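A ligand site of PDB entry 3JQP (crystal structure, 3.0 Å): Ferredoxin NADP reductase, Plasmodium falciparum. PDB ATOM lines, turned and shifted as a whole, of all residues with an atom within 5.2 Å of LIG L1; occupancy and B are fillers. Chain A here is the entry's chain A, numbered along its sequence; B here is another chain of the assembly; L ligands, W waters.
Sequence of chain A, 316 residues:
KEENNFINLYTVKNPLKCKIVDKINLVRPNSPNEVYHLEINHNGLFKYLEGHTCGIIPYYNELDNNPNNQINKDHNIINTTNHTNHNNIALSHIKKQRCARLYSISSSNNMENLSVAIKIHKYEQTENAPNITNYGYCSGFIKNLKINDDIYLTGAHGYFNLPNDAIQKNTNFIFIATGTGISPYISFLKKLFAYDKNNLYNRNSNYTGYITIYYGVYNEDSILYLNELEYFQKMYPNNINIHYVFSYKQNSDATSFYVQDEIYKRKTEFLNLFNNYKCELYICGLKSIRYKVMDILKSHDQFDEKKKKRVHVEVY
N of Cys 138 lies within hydrogen-bond range of O13 of LIG L1, 2.5 Å away.
The backbone NH (N) of Tyr 137 is in hydrogen-bond range of an oxygen (O15) of LIG L1.
An oxygen (O13) of LIG L1 sits at hydrogen-bond distance from the backbone NH (N) of Ser 139 (3.0 Å).
O14 of LIG L1 sits at hydrogen-bond distance from OG of Ser 139 (2.8 Å).
The backbone carbonyl oxygen (O) of Leu 102 of chain A sits close to an oxygen (O9) of LIG L1 (3.3 Å).
The backbone NH (N) of Lys 119 is in hydrogen-bond range of an oxygen (O7) of LIG L1, 3.1 Å away.
The side-chain hydroxyl of Tyr 103 is in hydrogen-bond range of an oxygen (O10) of LIG L1 (3.1 Å).
The guanidinium group of Arg 101 is in salt-bridge range of an oxygen (O1) of LIG L1 (3.1 Å).
The backbone carbonyl oxygen (O) of Ala 117 sits at hydrogen-bond distance from a nitrogen (N7) of LIG L1, at 3.1 Å.
The side-chain hydroxyl of Thr 180 is in hydrogen-bond range of a nitrogen (N7) of LIG L1 (3.2 Å).
A ring nitrogen (ND1) of His 121 lies within hydrogen-bond range of an oxygen (O5) of LIG L1, at 3.2 Å.
The side-chain hydroxyl of Tyr 123 lies within hydrogen-bond range of a nitrogen (N2) of LIG L1 (3.2 Å).
OH of Tyr 316 of chain A lies close to N8 of LIG L1, 3.4 Å away.
The backbone NH (N) of Ser 104 lies within hydrogen-bond range of an oxygen (O8) of LIG L1 (3.4 Å).
O of Leu 102 of chain B is in hydrogen-bond range of O9 of LG2 L2 (3.2 Å).
CG2 of Thr 53 touches C15 of LIG L1 (3.97 Å).
Ile 118 touches LIG L1.
Lys 122 touches LIG L1 (O to O6, 3.6 Å).
Gly 136 touches LIG L1.
OE2 of Glu 314 of chain A touches C17 of LIG L1, at 3.2 Å.
CD1 of Leu 102 of chain B touches N3 of LIG L1, 3.6 Å away.
Hydrophobic or aromatic side chains within 4 Å of LIG L1: Tyr 103, His 121, Tyr 123, Tyr 137, Tyr 316 of chain A and Leu 102 of chain B.
19 residues have an atom within 4 Å of LIG L1: Thr 53, Arg 101, Leu 102 of chain A, Tyr 103, Ser 104, Ala 117, Ile 118, Lys 119, His 121, Lys 122, Tyr 123, Gly 136, Tyr 137, Cys 138, Ser 139, Thr 180, Glu 314 of chain A, Tyr 316 of chain A and Leu 102 of chain B.
The nearest printed residue that does not touch LIG L1 is Val 315 of chain B (4.3 Å).
The side-chain sulfur (SG) of Cys 138 is in hydrogen-bond range of the side-chain hydroxyl (OH) of Tyr 103 (2.9 Å).
OG of Ser 139 lies within hydrogen-bond range of N of His 121.
The side-chain hydroxyl (OH) of Tyr 316 of chain A sits at hydrogen-bond distance from the side-chain hydroxyl (OG1) of Thr 180, 2.7 Å away.
N of Gly 136 sits at hydrogen-bond distance from O of His 121 (3.0 Å).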
ATOM      1  N   THR A  53      26.109   7.718  -9.124  1.00  0.00           N
ATOM      2  CA  THR A  53      24.817   7.869  -8.470  1.00  0.00           C
ATOM      3  C   THR A  53      24.873   9.080  -7.568  1.00  0.00           C
ATOM      4  O   THR A  53      25.958   9.588  -7.264  1.00  0.00           O
ATOM      5  CB  THR A  53      24.436   6.646  -7.627  1.00  0.00           C
ATOM      6  OG1 THR A  53      25.310   6.544  -6.492  1.00  0.00           O
ATOM      7  CG2 THR A  53      24.527   5.369  -8.444  1.00  0.00           C
ATOM      8  N   ARG A 101      19.388   7.193   0.114  1.00  0.00           N
ATOM      9  CA  ARG A 101      19.348   6.083  -0.832  1.00  0.00           C
ATOM     10  C   ARG A 101      20.053   6.543  -2.087  1.00  0.00           C
ATOM     11  O   ARG A 101      20.101   7.738  -2.374  1.00  0.00           O
ATOM     12  CB  ARG A 101      17.909   5.699  -1.180  1.00  0.00           C
ATOM     13  CG  ARG A 101      16.949   5.667  -0.013  1.00  0.00           C
ATOM     14  CD  ARG A 101      17.227   4.533   0.944  1.00  0.00           C
ATOM     15  NE  ARG A 101      16.074   4.310   1.802  1.00  0.00           N
ATOM     16  CZ  ARG A 101      16.125   3.855   3.052  1.00  0.00           C
ATOM     17  NH1 ARG A 101      17.299   3.575   3.598  1.00  0.00           N
ATOM     18  NH2 ARG A 101      15.013   3.688   3.742  1.00  0.00           N
ATOM     19  N   LEU A 102      20.594   5.602  -2.856  1.00  0.00           N
ATOM     20  CA  LEU A 102      21.333   5.972  -4.052  1.00  0.00           C
ATOM     21  C   LEU A 102      20.493   5.790  -5.316  1.00  0.00           C
ATOM     22  O   LEU A 102      19.794   4.787  -5.473  1.00  0.00           O
ATOM     23  CB  LEU A 102      22.639   5.171  -4.146  1.00  0.00           C
ATOM     24  CG  LEU A 102      23.646   5.373  -3.018  1.00  0.00           C
ATOM     25  CD1 LEU A 102      24.802   4.384  -3.139  1.00  0.00           C
ATOM     26  CD2 LEU A 102      24.166   6.810  -2.971  1.00  0.00           C
ATOM     27  N   TYR A 103      20.561   6.768  -6.198  1.00  0.00           N
ATOM     28  CA  TYR A 103      19.860   6.690  -7.471  1.00  0.00           C
ATOM     29  C   TYR A 103      20.777   7.079  -8.625  1.00  0.00           C
ATOM     30  O   TYR A 103      21.442   8.126  -8.588  1.00  0.00           O
ATOM     31  CB  TYR A 103      18.596   7.554  -7.448  1.00  0.00           C
ATOM     32  CG  TYR A 103      17.638   7.141  -6.349  1.00  0.00           C
ATOM     33  CD1 TYR A 103      17.658   7.774  -5.112  1.00  0.00           C
ATOM     34  CD2 TYR A 103      16.723   6.119  -6.549  1.00  0.00           C
ATOM     35  CE1 TYR A 103      16.793   7.395  -4.101  1.00  0.00           C
ATOM     36  CE2 TYR A 103      15.840   5.726  -5.545  1.00  0.00           C
ATOM     37  CZ  TYR A 103      15.887   6.373  -4.321  1.00  0.00           C
ATOM     38  OH  TYR A 103      15.028   5.998  -3.318  1.00  0.00           O
ATOM     39  N   SER A 104      20.833   6.212  -9.634  1.00  0.00           N
ATOM     40  CA  SER A 104      21.656   6.427 -10.807  1.00  0.00           C
ATOM     41  C   SER A 104      21.233   7.670 -11.588  1.00  0.00           C
ATOM     42  O   SER A 104      20.065   7.837 -11.921  1.00  0.00           O
ATOM     43  CB  SER A 104      21.592   5.209 -11.731  1.00  0.00           C
ATOM     44  OG  SER A 104      22.405   4.147 -11.246  1.00  0.00           O
ATOM     45  N   ALA A 117      15.783   8.688 -12.070  1.00  0.00           N
ATOM     46  CA  ALA A 117      14.542   7.921 -12.190  1.00  0.00           C
ATOM     47  C   ALA A 117      14.300   7.067 -10.948  1.00  0.00           C
ATOM     48  O   ALA A 117      15.173   6.325 -10.513  1.00  0.00           O
ATOM     49  CB  ALA A 117      14.585   7.041 -13.426  1.00  0.00           C
ATOM     50  N   ILE A 118      13.096   7.163 -10.378  1.00  0.00           N
ATOM     51  CA  ILE A 118      12.797   6.441  -9.137  1.00  0.00           C
ATOM     52  C   ILE A 118      11.550   5.560  -9.199  1.00  0.00           C
ATOM     53  O   ILE A 118      10.435   6.045  -9.417  1.00  0.00           O
ATOM     54  CB  ILE A 118      12.642   7.396  -7.943  1.00  0.00           C
ATOM     55  CG1 ILE A 118      13.866   8.308  -7.843  1.00  0.00           C
ATOM     56  CG2 ILE A 118      12.449   6.596  -6.653  1.00  0.00           C
ATOM     57  CD1 ILE A 118      13.580   9.606  -7.061  1.00  0.00           C
ATOM     58  N   LYS A 119      11.748   4.256  -9.003  1.00  0.00           N
ATOM     59  CA  LYS A 119      10.666   3.301  -8.853  1.00  0.00           C
ATOM     60  C   LYS A 119      10.059   3.442  -7.456  1.00  0.00           C
ATOM     61  O   LYS A 119      10.785   3.550  -6.468  1.00  0.00           O
ATOM     62  CB  LYS A 119      11.176   1.874  -9.079  1.00  0.00           C
ATOM     63  CG  LYS A 119      10.351   0.799  -8.383  1.00  0.00           C
ATOM     64  CD  LYS A 119      10.504  -0.563  -9.053  1.00  0.00           C
ATOM     65  CE  LYS A 119       9.658  -1.603  -8.343  1.00  0.00           C
ATOM     66  NZ  LYS A 119       9.197  -2.712  -9.255  1.00  0.00           N
ATOM     67  N   HIS A 121       8.406   1.871  -4.489  1.00  0.00           N
ATOM     68  CA  HIS A 121       8.216   0.549  -3.890  1.00  0.00           C
ATOM     69  C   HIS A 121       7.019   0.497  -2.952  1.00  0.00           C
ATOM     70  O   HIS A 121       6.870   1.344  -2.072  1.00  0.00           O
ATOM     71  CB  HIS A 121       9.490   0.132  -3.156  1.00  0.00           C
ATOM     72  CG  HIS A 121      10.678   0.008  -4.055  1.00  0.00           C
ATOM     73  ND1 HIS A 121      11.118  -1.211  -4.530  1.00  0.00           N
ATOM     74  CD2 HIS A 121      11.501   0.938  -4.598  1.00  0.00           C
ATOM     75  CE1 HIS A 121      12.167  -1.025  -5.309  1.00  0.00           C
ATOM     76  NE2 HIS A 121      12.417   0.270  -5.377  1.00  0.00           N
ATOM     77  N   LYS A 122       6.182  -0.515  -3.145  1.00  0.00           N
ATOM     78  CA  LYS A 122       4.952  -0.649  -2.364  1.00  0.00           C
ATOM     79  C   LYS A 122       4.852  -2.000  -1.636  1.00  0.00           C
ATOM     80  O   LYS A 122       5.555  -2.955  -1.954  1.00  0.00           O
ATOM     81  CB  LYS A 122       3.733  -0.468  -3.268  1.00  0.00           C
ATOM     82  CG  LYS A 122       3.636   0.898  -3.915  1.00  0.00           C
ATOM     83  CD  LYS A 122       2.882   0.821  -5.239  1.00  0.00           C
ATOM     84  CE  LYS A 122       3.222   2.002  -6.131  1.00  0.00           C
ATOM     85  NZ  LYS A 122       2.868   1.755  -7.560  1.00  0.00           N
ATOM     86  N   TYR A 123       3.962  -2.040  -0.648  1.00  0.00           N
ATOM     87  CA  TYR A 123       3.571  -3.277   0.023  1.00  0.00           C
ATOM     88  C   TYR A 123       2.239  -3.074   0.727  1.00  0.00           C
ATOM     89  O   TYR A 123       1.897  -1.961   1.114  1.00  0.00           O
ATOM     90  CB  TYR A 123       4.649  -3.783   0.983  1.00  0.00           C
ATOM     91  CG  TYR A 123       5.161  -2.770   1.991  1.00  0.00           C
ATOM     92  CD1 TYR A 123       4.718  -2.784   3.307  1.00  0.00           C
ATOM     93  CD2 TYR A 123       6.107  -1.823   1.622  1.00  0.00           C
ATOM     94  CE1 TYR A 123       5.197  -1.865   4.231  1.00  0.00           C
ATOM     95  CE2 TYR A 123       6.592  -0.900   2.538  1.00  0.00           C
ATOM     96  CZ  TYR A 123       6.130  -0.929   3.848  1.00  0.00           C
ATOM     97  OH  TYR A 123       6.604  -0.010   4.755  1.00  0.00           O
ATOM     98  N   GLY A 136       7.626   2.612   0.581  1.00  0.00           N
ATOM     99  CA  GLY A 136       9.001   2.635   1.075  1.00  0.00           C
ATOM    100  C   GLY A 136       9.325   3.987   1.681  1.00  0.00           C
ATOM    101  O   GLY A 136       8.551   4.936   1.537  1.00  0.00           O
ATOM    102  N   TYR A 137      10.467   4.101   2.359  1.00  0.00           N
ATOM    103  CA  TYR A 137      10.839   5.363   3.020  1.00  0.00           C
ATOM    104  C   TYR A 137      11.098   6.503   2.024  1.00  0.00           C
ATOM    105  O   TYR A 137      10.512   7.577   2.140  1.00  0.00           O
ATOM    106  CB  TYR A 137      12.042   5.154   3.952  1.00  0.00           C
ATOM    107  CG  TYR A 137      12.463   6.390   4.754  1.00  0.00           C
ATOM    108  CD1 TYR A 137      11.565   7.085   5.558  1.00  0.00           C
ATOM    109  CD2 TYR A 137      13.785   6.824   4.740  1.00  0.00           C
ATOM    110  CE1 TYR A 137      11.964   8.197   6.296  1.00  0.00           C
ATOM    111  CE2 TYR A 137      14.195   7.927   5.468  1.00  0.00           C
ATOM    112  CZ  TYR A 137      13.279   8.611   6.242  1.00  0.00           C
ATOM    113  OH  TYR A 137      13.689   9.714   6.970  1.00  0.00           O
ATOM    114  N   CYS A 138      11.991   6.273   1.062  1.00  0.00           N
ATOM    115  CA  CYS A 138      12.310   7.289   0.073  1.00  0.00           C
ATOM    116  C   CYS A 138      11.261   7.324  -1.034  1.00  0.00           C
ATOM    117  O   CYS A 138      10.981   8.364  -1.642  1.00  0.00           O
ATOM    118  CB  CYS A 138      13.687   7.033  -0.520  1.00  0.00           C
ATOM    119  SG  CYS A 138      14.248   8.297  -1.678  1.00  0.00           S
ATOM    120  N   SER A 139      10.675   6.153  -1.286  1.00  0.00           N
ATOM    121  CA  SER A 139       9.607   6.027  -2.248  1.00  0.00           C
ATOM    122  C   SER A 139       8.480   6.958  -1.806  1.00  0.00           C
ATOM    123  O   SER A 139       8.099   7.864  -2.538  1.00  0.00           O
ATOM    124  CB  SER A 139       9.104   4.586  -2.312  1.00  0.00           C
ATOM    125  OG  SER A 139      10.156   3.685  -2.621  1.00  0.00           O
ATOM    126  N   THR A 180      15.110  -0.004 -13.564  1.00  0.00           N
ATOM    127  CA  THR A 180      15.768   1.284 -13.347  1.00  0.00           C
ATOM    128  C   THR A 180      17.261   1.245 -13.672  1.00  0.00           C
ATOM    129  O   THR A 180      17.904   2.288 -13.799  1.00  0.00           O
ATOM    130  CB  THR A 180      15.561   1.786 -11.899  1.00  0.00           C
ATOM    131  OG1 THR A 180      16.367   1.019 -11.008  1.00  0.00           O
ATOM    132  CG2 THR A 180      14.097   1.658 -11.492  1.00  0.00           C
ATOM    133  N   SER A 183      19.141   3.568 -16.266  1.00  0.00           N
ATOM    134  CA  SER A 183      19.560   4.949 -16.027  1.00  0.00           C
ATOM    135  C   SER A 183      21.012   5.266 -16.430  1.00  0.00           C
ATOM    136  O   SER A 183      21.249   6.160 -17.246  1.00  0.00           O
ATOM    137  CB  SER A 183      19.289   5.383 -14.579  1.00  0.00           C
ATOM    138  OG  SER A 183      18.008   5.976 -14.452  1.00  0.00           O
ATOM    139  N   GLU A 314      27.242  -3.394 -11.250  1.00  0.00           N
ATOM    140  CA  GLU A 314      26.621  -2.601 -10.201  1.00  0.00           C
ATOM    141  C   GLU A 314      25.180  -3.068 -10.037  1.00  0.00           C
ATOM    142  O   GLU A 314      24.287  -2.628 -10.767  1.00  0.00           O
ATOM    143  CB  GLU A 314      26.666  -1.115 -10.544  1.00  0.00           C
ATOM    144  CG  GLU A 314      26.050  -0.203  -9.486  1.00  0.00           C
ATOM    145  CD  GLU A 314      26.072   1.261  -9.895  1.00  0.00           C
ATOM    146  OE1 GLU A 314      25.603   1.589 -11.003  1.00  0.00           O
ATOM    147  OE2 GLU A 314      26.553   2.083  -9.084  1.00  0.00           O
ATOM    148  N   VAL A 315      24.957  -3.977  -9.098  1.00  0.00           N
ATOM    149  CA  VAL A 315      23.629  -4.564  -8.901  1.00  0.00           C
ATOM    150  C   VAL A 315      23.020  -4.287  -7.517  1.00  0.00           C
ATOM    151  O   VAL A 315      23.717  -3.976  -6.555  1.00  0.00           O
ATOM    152  CB  VAL A 315      23.650  -6.091  -9.191  1.00  0.00           C
ATOM    153  CG1 VAL A 315      23.802  -6.342 -10.686  1.00  0.00           C
ATOM    154  CG2 VAL A 315      24.763  -6.786  -8.405  1.00  0.00           C
ATOM    155  N   TYR A 316      21.688  -4.389  -7.453  1.00  0.00           N
ATOM    156  CA  TYR A 316      20.933  -4.120  -6.229  1.00  0.00           C
ATOM    157  C   TYR A 316      19.509  -4.675  -6.321  1.00  0.00           C
ATOM    158  O   TYR A 316      18.904  -4.681  -7.398  1.00  0.00           O
ATOM    159  CB  TYR A 316      20.880  -2.607  -5.942  1.00  0.00           C
ATOM    160  CG  TYR A 316      20.354  -1.779  -7.093  1.00  0.00           C
ATOM    161  CD1 TYR A 316      19.008  -1.444  -7.178  1.00  0.00           C
ATOM    162  CD2 TYR A 316      21.211  -1.326  -8.098  1.00  0.00           C
ATOM    163  CE1 TYR A 316      18.529  -0.682  -8.236  1.00  0.00           C
ATOM    164  CE2 TYR A 316      20.726  -0.567  -9.149  1.00  0.00           C
ATOM    165  CZ  TYR A 316      19.386  -0.250  -9.213  1.00  0.00           C
ATOM    166  OH  TYR A 316      18.911   0.512 -10.254  1.00  0.00           O
ATOM    167  N   LEU B 102      15.443  -4.240   8.223  1.00  0.00           N
ATOM    168  CA  LEU B 102      14.615  -5.253   8.868  1.00  0.00           C
ATOM    169  C   LEU B 102      15.143  -6.631   8.547  1.00  0.00           C
ATOM    170  O   LEU B 102      15.685  -6.873   7.463  1.00  0.00           O
ATOM    171  CB  LEU B 102      13.169  -5.148   8.400  1.00  0.00           C
ATOM    172  CG  LEU B 102      12.401  -3.859   8.665  1.00  0.00           C
ATOM    173  CD1 LEU B 102      11.167  -3.821   7.773  1.00  0.00           C
ATOM    174  CD2 LEU B 102      12.005  -3.752  10.128  1.00  0.00           C
ATOM    175  N   GLU B 314       4.692 -11.532   1.333  1.00  0.00           N
ATOM    176  CA  GLU B 314       5.694 -10.652   1.894  1.00  0.00           C
ATOM    177  C   GLU B 314       6.856 -10.691   0.940  1.00  0.00           C
ATOM    178  O   GLU B 314       7.347 -11.775   0.592  1.00  0.00           O
ATOM    179  CB  GLU B 314       6.120 -11.126   3.281  1.00  0.00           C
ATOM    180  CG  GLU B 314       7.163 -10.246   3.951  1.00  0.00           C
ATOM    181  CD  GLU B 314       7.548 -10.737   5.326  1.00  0.00           C
ATOM    182  OE1 GLU B 314       7.015 -11.776   5.757  1.00  0.00           O
ATOM    183  OE2 GLU B 314       8.397 -10.092   5.981  1.00  0.00           O
ATOM    184  N   VAL B 315       7.318  -9.532   0.492  1.00  0.00           N
ATOM    185  CA  VAL B 315       8.444  -9.519  -0.449  1.00  0.00           C
ATOM    186  C   VAL B 315       9.454  -8.390  -0.208  1.00  0.00           C
ATOM    187  O   VAL B 315       9.080  -7.228  -0.003  1.00  0.00           O
ATOM    188  CB  VAL B 315       8.003  -9.513  -1.933  1.00  0.00           C
ATOM    189  CG1 VAL B 315       7.163 -10.741  -2.248  1.00  0.00           C
ATOM    190  CG2 VAL B 315       7.238  -8.228  -2.274  1.00  0.00           C
ATOM    191  N   TYR B 316      10.724  -8.763  -0.234  1.00  0.00           N
ATOM    192  CA  TYR B 316      11.829  -7.846  -0.018  1.00  0.00           C
ATOM    193  C   TYR B 316      13.006  -8.252  -0.905  1.00  0.00           C
ATOM    194  O   TYR B 316      13.301  -7.598  -1.905  1.00  0.00           O
ATOM    195  CB  TYR B 316      12.245  -7.838   1.456  1.00  0.00           C
ATOM    196  CG  TYR B 316      12.798  -9.161   1.958  1.00  0.00           C
ATOM    197  CD1 TYR B 316      14.133  -9.492   1.774  1.00  0.00           C
ATOM    198  CD2 TYR B 316      11.985 -10.069   2.625  1.00  0.00           C
ATOM    199  CE1 TYR B 316      14.645 -10.701   2.238  1.00  0.00           C
ATOM    200  CE2 TYR B 316      12.484 -11.277   3.094  1.00  0.00           C
ATOM    201  CZ  TYR B 316      13.824 -11.588   2.897  1.00  0.00           C
ATOM    202  OH  TYR B 316      14.336 -12.781   3.356  1.00  0.00           O
HETATM  203  P1  LIG L   1      12.989   1.152   2.103  1.00  0.00           P
HETATM  204  O1  LIG L   1      14.463   1.081   2.224  1.00  0.00           O
HETATM  205  O2  LIG L   1      12.142   0.999   3.304  1.00  0.00           O
HETATM  206  O3  LIG L   1      12.534  -0.005   1.078  1.00  0.00           O
HETATM  207  C1  LIG L   1      12.677  -1.377   1.518  1.00  0.00           C
HETATM  208  C2  LIG L   1      12.041  -2.368   0.514  1.00  0.00           C
HETATM  209  O4  LIG L   1      11.208  -3.336   1.203  1.00  0.00           O
HETATM  210  C3  LIG L   1      11.111  -1.701  -0.487  1.00  0.00           C
HETATM  211  O5  LIG L   1      10.999  -2.533  -1.637  1.00  0.00           O
HETATM  212  C4  LIG L   1       9.780  -1.655   0.259  1.00  0.00           C
HETATM  213  O6  LIG L   1       8.709  -1.866  -0.668  1.00  0.00           O
HETATM  214  C5  LIG L   1       9.838  -2.849   1.216  1.00  0.00           C
HETATM  215  N1  LIG L   1       9.504  -2.541   2.636  1.00  0.00           N
HETATM  216  C6  LIG L   1       9.864  -1.484   3.360  1.00  0.00           C
HETATM  217  N2  LIG L   1       9.366  -1.604   4.599  1.00  0.00           N
HETATM  218  C7  LIG L   1       8.700  -2.755   4.656  1.00  0.00           C
HETATM  219  C8  LIG L   1       7.985  -3.415   5.647  1.00  0.00           C
HETATM  220  N3  LIG L   1       7.862  -2.898   6.858  1.00  0.00           N
HETATM  221  N4  LIG L   1       7.409  -4.599   5.355  1.00  0.00           N
HETATM  222  C9  LIG L   1       7.519  -5.132   4.153  1.00  0.00           C
HETATM  223  N5  LIG L   1       8.200  -4.530   3.188  1.00  0.00           N
HETATM  224  C10 LIG L   1       8.791  -3.352   3.409  1.00  0.00           C
HETATM  225  N6  LIG L   1      16.420   2.566  -7.184  1.00  0.00           N
HETATM  226  C11 LIG L   1      15.638   3.114  -8.205  1.00  0.00           C
HETATM  227  O7  LIG L   1      14.416   3.073  -8.112  1.00  0.00           O
HETATM  228  N7  LIG L   1      16.260   3.706  -9.309  1.00  0.00           N
HETATM  229  C12 LIG L   1      17.659   3.746  -9.384  1.00  0.00           C
HETATM  230  O8  LIG L   1      18.198   4.269 -10.355  1.00  0.00           O
HETATM  231  C13 LIG L   1      18.432   3.202  -8.367  1.00  0.00           C
HETATM  232  N8  LIG L   1      19.829   3.233  -8.447  1.00  0.00           N
HETATM  233  C14 LIG L   1      20.591   2.540  -7.499  1.00  0.00           C
HETATM  234  C15 LIG L   1      21.971   2.434  -7.646  1.00  0.00           C
HETATM  235  C16 LIG L   1      22.726   1.745  -6.700  1.00  0.00           C
HETATM  236  C17 LIG L   1      24.250   1.632  -6.880  1.00  0.00           C
HETATM  237  C18 LIG L   1      22.109   1.157  -5.604  1.00  0.00           C
HETATM  238  C19 LIG L   1      22.934   0.404  -4.562  1.00  0.00           C
HETATM  239  C20 LIG L   1      20.732   1.271  -5.452  1.00  0.00           C
HETATM  240  C21 LIG L   1      19.972   1.956  -6.390  1.00  0.00           C
HETATM  241  N9  LIG L   1      18.587   2.058  -6.235  1.00  0.00           N
HETATM  242  C22 LIG L   1      17.810   2.610  -7.263  1.00  0.00           C
HETATM  243  C23 LIG L   1      17.935   1.578  -4.991  1.00  0.00           C
HETATM  244  C24 LIG L   1      17.103   2.670  -4.314  1.00  0.00           C
HETATM  245  O9  LIG L   1      17.875   3.269  -3.275  1.00  0.00           O
HETATM  246  C25 LIG L   1      15.781   2.124  -3.748  1.00  0.00           C
HETATM  247  O10 LIG L   1      14.700   3.029  -3.986  1.00  0.00           O
HETATM  248  C26 LIG L   1      15.876   1.897  -2.249  1.00  0.00           C
HETATM  249  O11 LIG L   1      16.785   0.817  -1.995  1.00  0.00           O
HETATM  250  C27 LIG L   1      14.489   1.573  -1.686  1.00  0.00           C
HETATM  251  O12 LIG L   1      14.248   2.289  -0.473  1.00  0.00           O
HETATM  252  P2  LIG L   1      12.788   2.879  -0.157  1.00  0.00           P
HETATM  253  O13 LIG L   1      12.838   4.350  -0.266  1.00  0.00           O
HETATM  254  O14 LIG L   1      11.773   2.116  -0.933  1.00  0.00           O
HETATM  255  O15 LIG L   1      12.569   2.545   1.411  1.00  0.00           O
HETATM  256  P1  LG2 L   2      22.515  -1.464   1.665  1.00  0.00           P
HETATM  257  O1  LG2 L   2      21.053  -1.252   1.714  1.00  0.00           O
HETATM  258  O2  LG2 L   2      23.424  -0.512   2.342  1.00  0.00           O
HETATM  259  O3  LG2 L   2      22.973  -1.567   0.116  1.00  0.00           O
HETATM  260  C1  LG2 L   2      21.995  -1.728  -0.905  1.00  0.00           C
HETATM  261  C2  LG2 L   2      22.347  -2.881  -1.846  1.00  0.00           C
HETATM  262  O4  LG2 L   2      23.131  -2.409  -2.974  1.00  0.00           O
HETATM  263  C3  LG2 L   2      23.204  -3.932  -1.127  1.00  0.00           C
HETATM  264  O5  LG2 L   2      22.855  -5.234  -1.633  1.00  0.00           O
HETATM  265  C4  LG2 L   2      24.650  -3.570  -1.484  1.00  0.00           C
HETATM  266  O6  LG2 L   2      25.358  -4.758  -1.848  1.00  0.00           O
HETATM  267  C5  LG2 L   2      24.549  -2.669  -2.721  1.00  0.00           C
HETATM  268  N1  LG2 L   2      25.182  -1.321  -2.598  1.00  0.00           N
HETATM  269  C6  LG2 L   2      24.969  -0.432  -1.624  1.00  0.00           C
HETATM  270  N2  LG2 L   2      25.692   0.667  -1.864  1.00  0.00           N
HETATM  271  C7  LG2 L   2      26.366   0.476  -2.987  1.00  0.00           C
HETATM  272  C8  LG2 L   2      27.256   1.264  -3.712  1.00  0.00           C
HETATM  273  N3  LG2 L   2      27.591   2.477  -3.272  1.00  0.00           N
HETATM  274  N4  LG2 L   2      27.770   0.775  -4.844  1.00  0.00           N
HETATM  275  C9  LG2 L   2      27.447  -0.428  -5.270  1.00  0.00           C
HETATM  276  N5  LG2 L   2      26.593  -1.197  -4.603  1.00  0.00           N
HETATM  277  C10 LG2 L   2      26.038  -0.775  -3.467  1.00  0.00           C
HETATM  278  N6  LG2 L   2      17.631  -9.447   4.611  1.00  0.00           N
HETATM  279  C11 LG2 L   2      18.174 -10.634   5.120  1.00  0.00           C
HETATM  280  O7  LG2 L   2      19.352 -10.928   4.896  1.00  0.00           O
HETATM  281  N7  LG2 L   2      17.389 -11.508   5.890  1.00  0.00           N
HETATM  282  C12 LG2 L   2      16.046 -11.177   6.148  1.00  0.00           C
HETATM  283  O8  LG2 L   2      15.330 -11.917   6.822  1.00  0.00           O
HETATM  284  C13 LG2 L   2      15.520  -9.999   5.645  1.00  0.00           C
HETATM  285  N8  LG2 L   2      14.186  -9.706   5.917  1.00  0.00           N
HETATM  286  C14 LG2 L   2      13.595  -8.571   5.360  1.00  0.00           C
HETATM  287  C15 LG2 L   2      12.246  -8.346   5.575  1.00  0.00           C
HETATM  288  C16 LG2 L   2      11.641  -7.227   5.027  1.00  0.00           C
HETATM  289  C17 LG2 L   2      10.149  -6.986   5.280  1.00  0.00           C
HETATM  290  C18 LG2 L   2      12.394  -6.338   4.268  1.00  0.00           C
HETATM  291  C19 LG2 L   2      11.744  -5.087   3.661  1.00  0.00           C
HETATM  292  C20 LG2 L   2      13.752  -6.568   4.057  1.00  0.00           C
HETATM  293  C21 LG2 L   2      14.356  -7.687   4.605  1.00  0.00           C
HETATM  294  N9  LG2 L   2      15.717  -7.938   4.386  1.00  0.00           N
HETATM  295  C22 LG2 L   2      16.292  -9.124   4.880  1.00  0.00           C
HETATM  296  C23 LG2 L   2      16.526  -6.947   3.638  1.00  0.00           C
HETATM  297  C24 LG2 L   2      17.535  -6.260   4.559  1.00  0.00           C
HETATM  298  O9  LG2 L   2      16.935  -5.103   5.154  1.00  0.00           O
HETATM  299  C25 LG2 L   2      18.811  -5.888   3.795  1.00  0.00           C
HETATM  300  O10 LG2 L   2      19.970  -6.305   4.540  1.00  0.00           O
HETATM  301  C26 LG2 L   2      18.930  -4.392   3.496  1.00  0.00           C
HETATM  302  O11 LG2 L   2      17.747  -3.909   2.846  1.00  0.00           O
HETATM  303  C27 LG2 L   2      20.165  -4.122   2.627  1.00  0.00           C
HETATM  304  O12 LG2 L   2      21.334  -4.563   3.314  1.00  0.00           O
HETATM  305  P2  LG2 L   2      22.494  -3.493   3.645  1.00  0.00           P
HETATM  306  O13 LG2 L   2      21.924  -2.411   4.476  1.00  0.00           O
HETATM  307  O14 LG2 L   2      23.682  -4.228   4.134  1.00  0.00           O
HETATM  308  O15 LG2 L   2      22.847  -2.949   2.169  1.00  0.00           O
HETATM  309  O   HOH W   1      14.266   0.383   5.569  1.00  0.00           O
